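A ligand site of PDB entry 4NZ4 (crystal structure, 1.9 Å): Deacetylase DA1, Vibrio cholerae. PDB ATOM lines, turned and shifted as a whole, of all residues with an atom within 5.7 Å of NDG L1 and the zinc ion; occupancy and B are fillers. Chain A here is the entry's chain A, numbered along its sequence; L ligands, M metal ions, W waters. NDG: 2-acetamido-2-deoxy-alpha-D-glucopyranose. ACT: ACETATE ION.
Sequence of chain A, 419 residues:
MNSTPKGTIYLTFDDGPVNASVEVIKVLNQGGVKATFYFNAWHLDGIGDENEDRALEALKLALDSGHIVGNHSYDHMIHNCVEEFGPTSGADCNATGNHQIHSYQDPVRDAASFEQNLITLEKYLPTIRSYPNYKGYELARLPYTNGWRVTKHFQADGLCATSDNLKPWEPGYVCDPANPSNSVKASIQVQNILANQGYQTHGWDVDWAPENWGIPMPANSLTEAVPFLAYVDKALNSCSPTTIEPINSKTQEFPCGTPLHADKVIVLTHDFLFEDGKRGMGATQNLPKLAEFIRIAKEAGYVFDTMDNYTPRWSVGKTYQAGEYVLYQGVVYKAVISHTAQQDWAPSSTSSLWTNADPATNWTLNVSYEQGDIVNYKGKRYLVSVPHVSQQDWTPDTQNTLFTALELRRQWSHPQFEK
The side-chain carboxylate (OD2) of Asp 15 is in hydrogen-bond range of an oxygen (O6) of NDG L1 (2.5 Å). The side-chain amide oxygen of Asn 94 sits at hydrogen-bond distance from an oxygen (O3) of NDG L1, at 2.7 Å. O7 of NDG L1 lies within hydrogen-bond range of NE of Arg 279, 2.7 Å away. NE2 of His 99 is in hydrogen-bond range of O4 of NDG L1 (3.4 Å).
The backbone carbonyl oxygen (O) of His 76 lies within hydrogen-bond range of the side-chain hydroxyl (OH) of Tyr 144, 3.1 Å away. NE2 of His 43 sits at hydrogen-bond distance from O of Asp 15, 2.7 Å away. The side-chain amide nitrogen (ND2) of Asn 40 sits at hydrogen-bond distance from the backbone carbonyl oxygen (O) of His 72, at 2.8 Å. The side-chain amide oxygen (OD1) of Asn 94 lies within hydrogen-bond range of a ring nitrogen (NE2) of His 99, 3.1 Å away. The side-chain amide nitrogen (ND2) of Asn 94 sits close to the backbone carbonyl oxygen (O) of Gly 90, 3.3 Å away. OE2 of Glu 50 is in salt-bridge range of NH2 of Arg 279 (2.9 Å).
Trp 213 touches NDG L1 (CZ3 to C8, 3.8 Å). Phe 272 touches NDG L1. Hydrophobic or aromatic side chains within 4 Å of NDG L1: His 76, His 99, Trp 213 and Phe 272. Within 4 Å of NDG L1: Asp 15, His 76, Asn 94, His 99, Trp 213, Phe 272 and Arg 279. Along chain A the residues within 4 Å of NDG L1 span positions 15 to 279.
Asp 14 touches the zinc ion (CB to ZN, 3.9 Å). His 270 touches the zinc ion (NE2 to ZN, 3.9 Å). Within 4 Å of the zinc ion: Asp 14, Asp 15, His 72, His 76 and His 270.
A ring nitrogen (NE2) of His 76 binds the zinc ion (1.9 Å). The zinc ion is bound by OD1 of Asp 15 (2.1 Å). An oxygen (OXT) of ACT L2 binds the zinc ion (2.1 Å). The zinc ion is bound by NE2 of His 72 (2.2 Å). The zinc ion is bound by an oxygen (O) of ACT L2. Water W2 binds the zinc ion, 2.4 Å away. The zinc ion has six donor atoms within binding distance.
Water W2 lies within hydrogen-bond range of the side-chain carboxylate (OD2) of Asp 15 (2.5 Å), a ring nitrogen (NE2) of His 270 (2.8 Å) and an oxygen (O5) of NDG L1 (3.3 Å). Water W5 lies within hydrogen-bond range of OE2 of Glu 50 (2.5 Å), O4 of NDG L1 (2.6 Å), ND2 of Asn 94 (2.8 Å) and O of Gly 48 (3.0 Å). Water W4 lies within hydrogen-bond range of an oxygen (O4) of NDG L1 (2.8 Å), the backbone carbonyl oxygen (O) of Gly 90 (2.8 Å), a ring nitrogen (NE2) of His 99 (2.8 Å) and the side-chain amide oxygen (OD1) of Asn 94 (3.2 Å). Water W3 lies within hydrogen-bond range of OD1 of Asn 40 (2.6 Å), NE2 of His 43 (2.9 Å), O6 of NDG L1 (2.9 Å), NE1 of Trp 42 (3.1 Å) and O of Asp 15 (3.4 Å). Water W6 lies within hydrogen-bond range of the side-chain carboxylate of Glu 50 (2.7 Å) and an oxygen (O6) of NDG L1 (2.9 Å).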
ATOM      1  N   ASP A  14      -9.596 -35.229 -17.893  1.00  0.00           N
ATOM      2  CA  ASP A  14     -10.355 -33.987 -17.937  1.00  0.00           C
ATOM      3  C   ASP A  14      -9.552 -32.759 -18.295  1.00  0.00           C
ATOM      4  O   ASP A  14      -8.395 -32.664 -17.947  1.00  0.00           O
ATOM      5  CB  ASP A  14     -11.033 -33.688 -16.577  1.00  0.00           C
ATOM      6  CG  ASP A  14     -12.188 -34.615 -16.301  1.00  0.00           C
ATOM      7  OD1 ASP A  14     -12.277 -35.667 -17.010  1.00  0.00           O
ATOM      8  OD2 ASP A  14     -12.985 -34.325 -15.363  1.00  0.00           O
ATOM      9  N   ASP A  15     -10.211 -31.824 -18.976  1.00  0.00           N
ATOM     10  CA  ASP A  15      -9.785 -30.435 -19.143  1.00  0.00           C
ATOM     11  C   ASP A  15      -8.888 -30.175 -20.360  1.00  0.00           C
ATOM     12  O   ASP A  15      -8.522 -29.048 -20.652  1.00  0.00           O
ATOM     13  CB  ASP A  15      -9.096 -29.855 -17.877  1.00  0.00           C
ATOM     14  CG  ASP A  15     -10.001 -29.792 -16.642  1.00  0.00           C
ATOM     15  OD1 ASP A  15     -11.053 -30.459 -16.545  1.00  0.00           O
ATOM     16  OD2 ASP A  15      -9.610 -29.083 -15.696  1.00  0.00           O
ATOM     17  N   ASN A  40     -12.900 -29.554 -22.654  1.00  0.00           N
ATOM     18  CA  ASN A  40     -13.342 -28.168 -22.671  1.00  0.00           C
ATOM     19  C   ASN A  40     -12.814 -27.491 -23.922  1.00  0.00           C
ATOM     20  O   ASN A  40     -11.610 -27.301 -24.061  1.00  0.00           O
ATOM     21  CB  ASN A  40     -12.776 -27.410 -21.467  1.00  0.00           C
ATOM     22  CG  ASN A  40     -13.157 -28.029 -20.165  1.00  0.00           C
ATOM     23  OD1 ASN A  40     -12.295 -28.398 -19.380  1.00  0.00           O
ATOM     24  ND2 ASN A  40     -14.461 -28.130 -19.898  1.00  0.00           N
ATOM     25  N   TRP A  42     -12.800 -24.519 -24.892  1.00  0.00           N
ATOM     26  CA  TRP A  42     -12.235 -23.175 -24.878  1.00  0.00           C
ATOM     27  C   TRP A  42     -10.725 -23.207 -25.141  1.00  0.00           C
ATOM     28  O   TRP A  42     -10.139 -22.220 -25.578  1.00  0.00           O
ATOM     29  CB  TRP A  42     -12.576 -22.405 -23.590  1.00  0.00           C
ATOM     30  CG  TRP A  42     -12.009 -22.915 -22.356  1.00  0.00           C
ATOM     31  CD1 TRP A  42     -11.657 -24.190 -22.070  1.00  0.00           C
ATOM     32  CD2 TRP A  42     -11.717 -22.144 -21.191  1.00  0.00           C
ATOM     33  NE1 TRP A  42     -11.148 -24.265 -20.794  1.00  0.00           N
ATOM     34  CE2 TRP A  42     -11.174 -23.014 -20.230  1.00  0.00           C
ATOM     35  CE3 TRP A  42     -11.845 -20.782 -20.864  1.00  0.00           C
ATOM     36  CZ2 TRP A  42     -10.773 -22.582 -18.957  1.00  0.00           C
ATOM     37  CZ3 TRP A  42     -11.449 -20.345 -19.608  1.00  0.00           C
ATOM     38  CH2 TRP A  42     -10.926 -21.247 -18.670  1.00  0.00           C
ATOM     39  N   HIS A  43     -10.093 -24.351 -24.952  1.00  0.00           N
ATOM     40  CA  HIS A  43      -8.666 -24.455 -25.254  1.00  0.00           C
ATOM     41  C   HIS A  43      -8.403 -24.338 -26.730  1.00  0.00           C
ATOM     42  O   HIS A  43      -7.343 -23.877 -27.144  1.00  0.00           O
ATOM     43  CB  HIS A  43      -8.094 -25.779 -24.751  1.00  0.00           C
ATOM     44  CG  HIS A  43      -8.145 -25.890 -23.270  1.00  0.00           C
ATOM     45  ND1 HIS A  43      -7.509 -24.999 -22.440  1.00  0.00           N
ATOM     46  CD2 HIS A  43      -8.795 -26.766 -22.470  1.00  0.00           C
ATOM     47  CE1 HIS A  43      -7.736 -25.331 -21.186  1.00  0.00           C
ATOM     48  NE2 HIS A  43      -8.525 -26.399 -21.173  1.00  0.00           N
ATOM     49  N   GLY A  48      -7.913 -20.652 -22.550  1.00  0.00           N
ATOM     50  CA  GLY A  48      -8.034 -21.509 -21.391  1.00  0.00           C
ATOM     51  C   GLY A  48      -6.862 -21.470 -20.428  1.00  0.00           C
ATOM     52  O   GLY A  48      -6.816 -22.263 -19.479  1.00  0.00           O
ATOM     53  N   GLU A  50      -3.775 -22.360 -20.656  1.00  0.00           N
ATOM     54  CA  GLU A  50      -2.838 -23.472 -20.671  1.00  0.00           C
ATOM     55  C   GLU A  50      -1.927 -23.364 -21.910  1.00  0.00           C
ATOM     56  O   GLU A  50      -2.149 -22.528 -22.795  1.00  0.00           O
ATOM     57  CB  GLU A  50      -3.597 -24.812 -20.666  1.00  0.00           C
ATOM     58  CG  GLU A  50      -4.585 -24.962 -19.515  1.00  0.00           C
ATOM     59  CD  GLU A  50      -3.914 -25.100 -18.176  1.00  0.00           C
ATOM     60  OE1 GLU A  50      -2.688 -25.357 -18.146  1.00  0.00           O
ATOM     61  OE2 GLU A  50      -4.634 -24.963 -17.163  1.00  0.00           O
ATOM     62  N   HIS A  72     -17.082 -31.791 -21.332  1.00  0.00           N
ATOM     63  CA  HIS A  72     -16.797 -31.277 -19.979  1.00  0.00           C
ATOM     64  C   HIS A  72     -17.257 -29.807 -19.833  1.00  0.00           C
ATOM     65  O   HIS A  72     -16.907 -29.118 -18.852  1.00  0.00           O
ATOM     66  CB  HIS A  72     -15.293 -31.425 -19.710  1.00  0.00           C
ATOM     67  CG  HIS A  72     -14.919 -31.364 -18.263  1.00  0.00           C
ATOM     68  ND1 HIS A  72     -15.715 -31.876 -17.265  1.00  0.00           N
ATOM     69  CD2 HIS A  72     -13.812 -30.876 -17.651  1.00  0.00           C
ATOM     70  CE1 HIS A  72     -15.133 -31.687 -16.091  1.00  0.00           C
ATOM     71  NE2 HIS A  72     -13.976 -31.082 -16.303  1.00  0.00           N
ATOM     72  N   HIS A  76     -15.366 -24.896 -18.622  1.00  0.00           N
ATOM     73  CA  HIS A  76     -15.216 -25.374 -17.248  1.00  0.00           C
ATOM     74  C   HIS A  76     -15.891 -24.447 -16.223  1.00  0.00           C
ATOM     75  O   HIS A  76     -15.460 -24.397 -15.081  1.00  0.00           O
ATOM     76  CB  HIS A  76     -13.718 -25.466 -16.891  1.00  0.00           C
ATOM     77  CG  HIS A  76     -13.394 -26.627 -16.029  1.00  0.00           C
ATOM     78  ND1 HIS A  76     -13.443 -26.575 -14.653  1.00  0.00           N
ATOM     79  CD2 HIS A  76     -13.005 -27.887 -16.352  1.00  0.00           C
ATOM     80  CE1 HIS A  76     -13.129 -27.771 -14.168  1.00  0.00           C
ATOM     81  NE2 HIS A  76     -12.846 -28.571 -15.184  1.00  0.00           N
ATOM     82  N   ILE A  78     -15.911 -21.290 -16.033  1.00  0.00           N
ATOM     83  CA  ILE A  78     -15.111 -20.159 -15.611  1.00  0.00           C
ATOM     84  C   ILE A  78     -15.930 -18.867 -15.730  1.00  0.00           C
ATOM     85  O   ILE A  78     -15.649 -17.892 -15.033  1.00  0.00           O
ATOM     86  CB  ILE A  78     -13.728 -20.118 -16.335  1.00  0.00           C
ATOM     87  CG1 ILE A  78     -12.658 -20.828 -15.494  1.00  0.00           C
ATOM     88  CG2 ILE A  78     -13.243 -18.697 -16.551  1.00  0.00           C
ATOM     89  CD1 ILE A  78     -12.748 -22.340 -15.464  1.00  0.00           C
ATOM     90  N   GLY A  90      -9.836 -17.285 -17.767  1.00  0.00           N
ATOM     91  CA  GLY A  90      -9.127 -18.446 -17.247  1.00  0.00           C
ATOM     92  C   GLY A  90      -7.965 -18.034 -16.349  1.00  0.00           C
ATOM     93  O   GLY A  90      -7.777 -18.569 -15.239  1.00  0.00           O
ATOM     94  N   ASN A  94      -7.688 -18.405 -12.420  1.00  0.00           N
ATOM     95  CA  ASN A  94      -6.451 -19.034 -11.951  1.00  0.00           C
ATOM     96  C   ASN A  94      -5.706 -18.129 -10.932  1.00  0.00           C
ATOM     97  O   ASN A  94      -5.100 -18.619  -9.996  1.00  0.00           O
ATOM     98  CB  ASN A  94      -5.510 -19.411 -13.122  1.00  0.00           C
ATOM     99  CG  ASN A  94      -5.894 -20.728 -13.816  1.00  0.00           C
ATOM    100  OD1 ASN A  94      -6.527 -21.607 -13.227  1.00  0.00           O
ATOM    101  ND2 ASN A  94      -5.475 -20.871 -15.060  1.00  0.00           N
ATOM    102  N   HIS A  99     -12.210 -21.206  -8.517  1.00  0.00           N
ATOM    103  CA  HIS A  99     -12.897 -22.166  -9.400  1.00  0.00           C
ATOM    104  C   HIS A  99     -14.105 -22.848  -8.744  1.00  0.00           C
ATOM    105  O   HIS A  99     -15.173 -22.953  -9.349  1.00  0.00           O
ATOM    106  CB  HIS A  99     -11.891 -23.223  -9.870  1.00  0.00           C
ATOM    107  CG  HIS A  99     -10.766 -22.655 -10.672  1.00  0.00           C
ATOM    108  ND1 HIS A  99      -9.594 -22.204 -10.095  1.00  0.00           N
ATOM    109  CD2 HIS A  99     -10.625 -22.458 -11.998  1.00  0.00           C
ATOM    110  CE1 HIS A  99      -8.783 -21.758 -11.037  1.00  0.00           C
ATOM    111  NE2 HIS A  99      -9.388 -21.885 -12.197  1.00  0.00           N
ATOM    112  N   PRO A 143     -17.936 -29.992 -14.498  1.00  0.00           N
ATOM    113  CA  PRO A 143     -16.806 -29.367 -13.798  1.00  0.00           C
ATOM    114  C   PRO A 143     -16.938 -29.433 -12.282  1.00  0.00           C
ATOM    115  O   PRO A 143     -18.023 -29.148 -11.765  1.00  0.00           O
ATOM    116  CB  PRO A 143     -16.886 -27.920 -14.292  1.00  0.00           C
ATOM    117  CG  PRO A 143     -17.354 -28.051 -15.725  1.00  0.00           C
ATOM    118  CD  PRO A 143     -18.381 -29.198 -15.652  1.00  0.00           C
ATOM    119  N   TYR A 144     -15.861 -29.873 -11.617  1.00  0.00           N
ATOM    120  CA  TYR A 144     -15.732 -29.877 -10.167  1.00  0.00           C
ATOM    121  C   TYR A 144     -16.552 -30.921  -9.445  1.00  0.00           C
ATOM    122  O   TYR A 144     -16.445 -31.071  -8.230  1.00  0.00           O
ATOM    123  CB  TYR A 144     -16.120 -28.517  -9.569  1.00  0.00           C
ATOM    124  CG  TYR A 144     -15.513 -27.399 -10.305  1.00  0.00           C
ATOM    125  CD1 TYR A 144     -14.134 -27.246 -10.338  1.00  0.00           C
ATOM    126  CD2 TYR A 144     -16.308 -26.515 -11.017  1.00  0.00           C
ATOM    127  CE1 TYR A 144     -13.577 -26.210 -11.026  1.00  0.00           C
ATOM    128  CE2 TYR A 144     -15.745 -25.493 -11.724  1.00  0.00           C
ATOM    129  CZ  TYR A 144     -14.374 -25.357 -11.735  1.00  0.00           C
ATOM    130  OH  TYR A 144     -13.818 -24.339 -12.447  1.00  0.00           O
ATOM    131  N   TRP A 213      -0.306 -30.667  -2.682  1.00  0.00           N
ATOM    132  CA  TRP A 213      -0.520 -29.475  -3.480  1.00  0.00           C
ATOM    133  C   TRP A 213       0.215 -28.279  -2.889  1.00  0.00           C
ATOM    134  O   TRP A 213       0.215 -27.202  -3.479  1.00  0.00           O
ATOM    135  CB  TRP A 213      -2.016 -29.142  -3.555  1.00  0.00           C
ATOM    136  CG  TRP A 213      -2.781 -29.881  -4.571  1.00  0.00           C
ATOM    137  CD1 TRP A 213      -3.653 -30.922  -4.360  1.00  0.00           C
ATOM    138  CD2 TRP A 213      -2.791 -29.639  -5.988  1.00  0.00           C
ATOM    139  NE1 TRP A 213      -4.202 -31.334  -5.557  1.00  0.00           N
ATOM    140  CE2 TRP A 213      -3.687 -30.559  -6.568  1.00  0.00           C
ATOM    141  CE3 TRP A 213      -2.124 -28.725  -6.818  1.00  0.00           C
ATOM    142  CZ2 TRP A 213      -3.933 -30.604  -7.949  1.00  0.00           C
ATOM    143  CZ3 TRP A 213      -2.386 -28.762  -8.199  1.00  0.00           C
ATOM    144  CH2 TRP A 213      -3.280 -29.706  -8.750  1.00  0.00           C
ATOM    145  N   HIS A 270      -6.086 -35.437 -14.983  1.00  0.00           N
ATOM    146  CA  HIS A 270      -6.045 -34.240 -15.781  1.00  0.00           C
ATOM    147  C   HIS A 270      -4.837 -34.234 -16.679  1.00  0.00           C
ATOM    148  O   HIS A 270      -3.723 -34.436 -16.215  1.00  0.00           O
ATOM    149  CB  HIS A 270      -6.032 -32.990 -14.877  1.00  0.00           C
ATOM    150  CG  HIS A 270      -7.315 -32.767 -14.124  1.00  0.00           C
ATOM    151  ND1 HIS A 270      -7.647 -33.458 -12.965  1.00  0.00           N
ATOM    152  CD2 HIS A 270      -8.328 -31.906 -14.333  1.00  0.00           C
ATOM    153  CE1 HIS A 270      -8.820 -33.045 -12.528  1.00  0.00           C
ATOM    154  NE2 HIS A 270      -9.251 -32.094 -13.329  1.00  0.00           N
ATOM    155  N   PHE A 272      -3.271 -31.863 -17.924  1.00  0.00           N
ATOM    156  CA  PHE A 272      -2.269 -30.860 -17.550  1.00  0.00           C
ATOM    157  C   PHE A 272      -1.280 -31.344 -16.484  1.00  0.00           C
ATOM    158  O   PHE A 272      -0.250 -30.699 -16.270  1.00  0.00           O
ATOM    159  CB  PHE A 272      -2.887 -29.504 -17.157  1.00  0.00           C
ATOM    160  CG  PHE A 272      -3.802 -29.521 -15.932  1.00  0.00           C
ATOM    161  CD1 PHE A 272      -3.345 -29.922 -14.680  1.00  0.00           C
ATOM    162  CD2 PHE A 272      -5.120 -29.086 -16.050  1.00  0.00           C
ATOM    163  CE1 PHE A 272      -4.200 -29.931 -13.586  1.00  0.00           C
ATOM    164  CE2 PHE A 272      -5.966 -29.077 -14.940  1.00  0.00           C
ATOM    165  CZ  PHE A 272      -5.506 -29.498 -13.720  1.00  0.00           C
ATOM    166  N   LYS A 278       3.985 -25.113 -15.631  1.00  0.00           N
ATOM    167  CA  LYS A 278       3.784 -24.271 -14.424  1.00  0.00           C
ATOM    168  C   LYS A 278       3.469 -25.069 -13.165  1.00  0.00           C
ATOM    169  O   LYS A 278       3.648 -24.565 -12.063  1.00  0.00           O
ATOM    170  CB  LYS A 278       2.702 -23.227 -14.643  1.00  0.00           C
ATOM    171  CG  LYS A 278       1.346 -23.792 -15.067  1.00  0.00           C
ATOM    172  CD  LYS A 278       0.334 -22.704 -15.153  1.00  0.00           C
ATOM    173  CE  LYS A 278      -0.854 -23.103 -16.021  1.00  0.00           C
ATOM    174  NZ  LYS A 278      -1.808 -21.970 -16.145  1.00  0.00           N
ATOM    175  N   ARG A 279       3.029 -26.303 -13.337  1.00  0.00           N
ATOM    176  CA  ARG A 279       2.617 -27.131 -12.220  1.00  0.00           C
ATOM    177  C   ARG A 279       3.712 -28.091 -11.790  1.00  0.00           C
ATOM    178  O   ARG A 279       3.587 -28.716 -10.749  1.00  0.00           O
ATOM    179  CB  ARG A 279       1.372 -27.913 -12.598  1.00  0.00           C
ATOM    180  CG  ARG A 279       0.130 -27.042 -12.702  1.00  0.00           C
ATOM    181  CD  ARG A 279      -1.090 -27.869 -13.107  1.00  0.00           C
ATOM    182  NE  ARG A 279      -2.260 -27.032 -13.352  1.00  0.00           N
ATOM    183  CZ  ARG A 279      -2.539 -26.433 -14.499  1.00  0.00           C
ATOM    184  NH1 ARG A 279      -1.756 -26.585 -15.576  1.00  0.00           N
ATOM    185  NH2 ARG A 279      -3.657 -25.722 -14.592  1.00  0.00           N
HETATM  186  C1  NDG L   1      -8.505 -26.785 -12.355  1.00  0.00           C
HETATM  187  C2  NDG L   1      -7.158 -26.038 -12.407  1.00  0.00           C
HETATM  188  C3  NDG L   1      -7.290 -24.663 -13.042  1.00  0.00           C
HETATM  189  C4  NDG L   1      -7.986 -24.780 -14.394  1.00  0.00           C
HETATM  190  C5  NDG L   1      -9.329 -25.478 -14.209  1.00  0.00           C
HETATM  191  C6  NDG L   1     -10.004 -25.689 -15.571  1.00  0.00           C
HETATM  192  C7  NDG L   1      -5.216 -26.249 -10.840  1.00  0.00           C
HETATM  193  C8  NDG L   1      -4.872 -26.156  -9.369  1.00  0.00           C
HETATM  194  O5  NDG L   1      -9.126 -26.778 -13.630  1.00  0.00           O
HETATM  195  O3  NDG L   1      -5.950 -24.242 -13.222  1.00  0.00           O
HETATM  196  O4  NDG L   1      -8.216 -23.485 -14.930  1.00  0.00           O
HETATM  197  O6  NDG L   1      -9.309 -26.673 -16.364  1.00  0.00           O
HETATM  198  O7  NDG L   1      -4.385 -26.535 -11.717  1.00  0.00           O
HETATM  199  N2  NDG L   1      -6.534 -25.968 -11.089  1.00  0.00           N
HETATM  200  O1  NDG L   1      -9.330 -26.191 -11.375  1.00  0.00           O
HETATM  201  C   ACT L   2     -13.319 -32.051 -13.169  1.00  0.00           C
HETATM  202  O   ACT L   2     -13.737 -30.882 -13.105  1.00  0.00           O
HETATM  203  OXT ACT L   2     -12.376 -32.314 -13.979  1.00  0.00           O
HETATM  204  CH3 ACT L   2     -13.966 -33.090 -12.309  1.00  0.00           C
HETATM  205 ZN    ZN M   1     -12.404 -30.409 -14.963  1.00  0.00          ZN
HETATM  206  O   HOH W   1     -10.809 -28.773 -10.862  1.00  0.00           O
HETATM  207  O   HOH W   2     -10.695 -29.713 -13.501  1.00  0.00           O
HETATM  208  O   HOH W   3     -10.412 -26.700 -19.056  1.00  0.00           O
HETATM  209  O   HOH W   4      -9.224 -20.907 -14.831  1.00  0.00           O
HETATM  210  O   HOH W   5      -6.282 -23.095 -16.625  1.00  0.00           O
HETATM  211  O   HOH W   6      -6.889 -26.203 -17.975  1.00  0.00           O
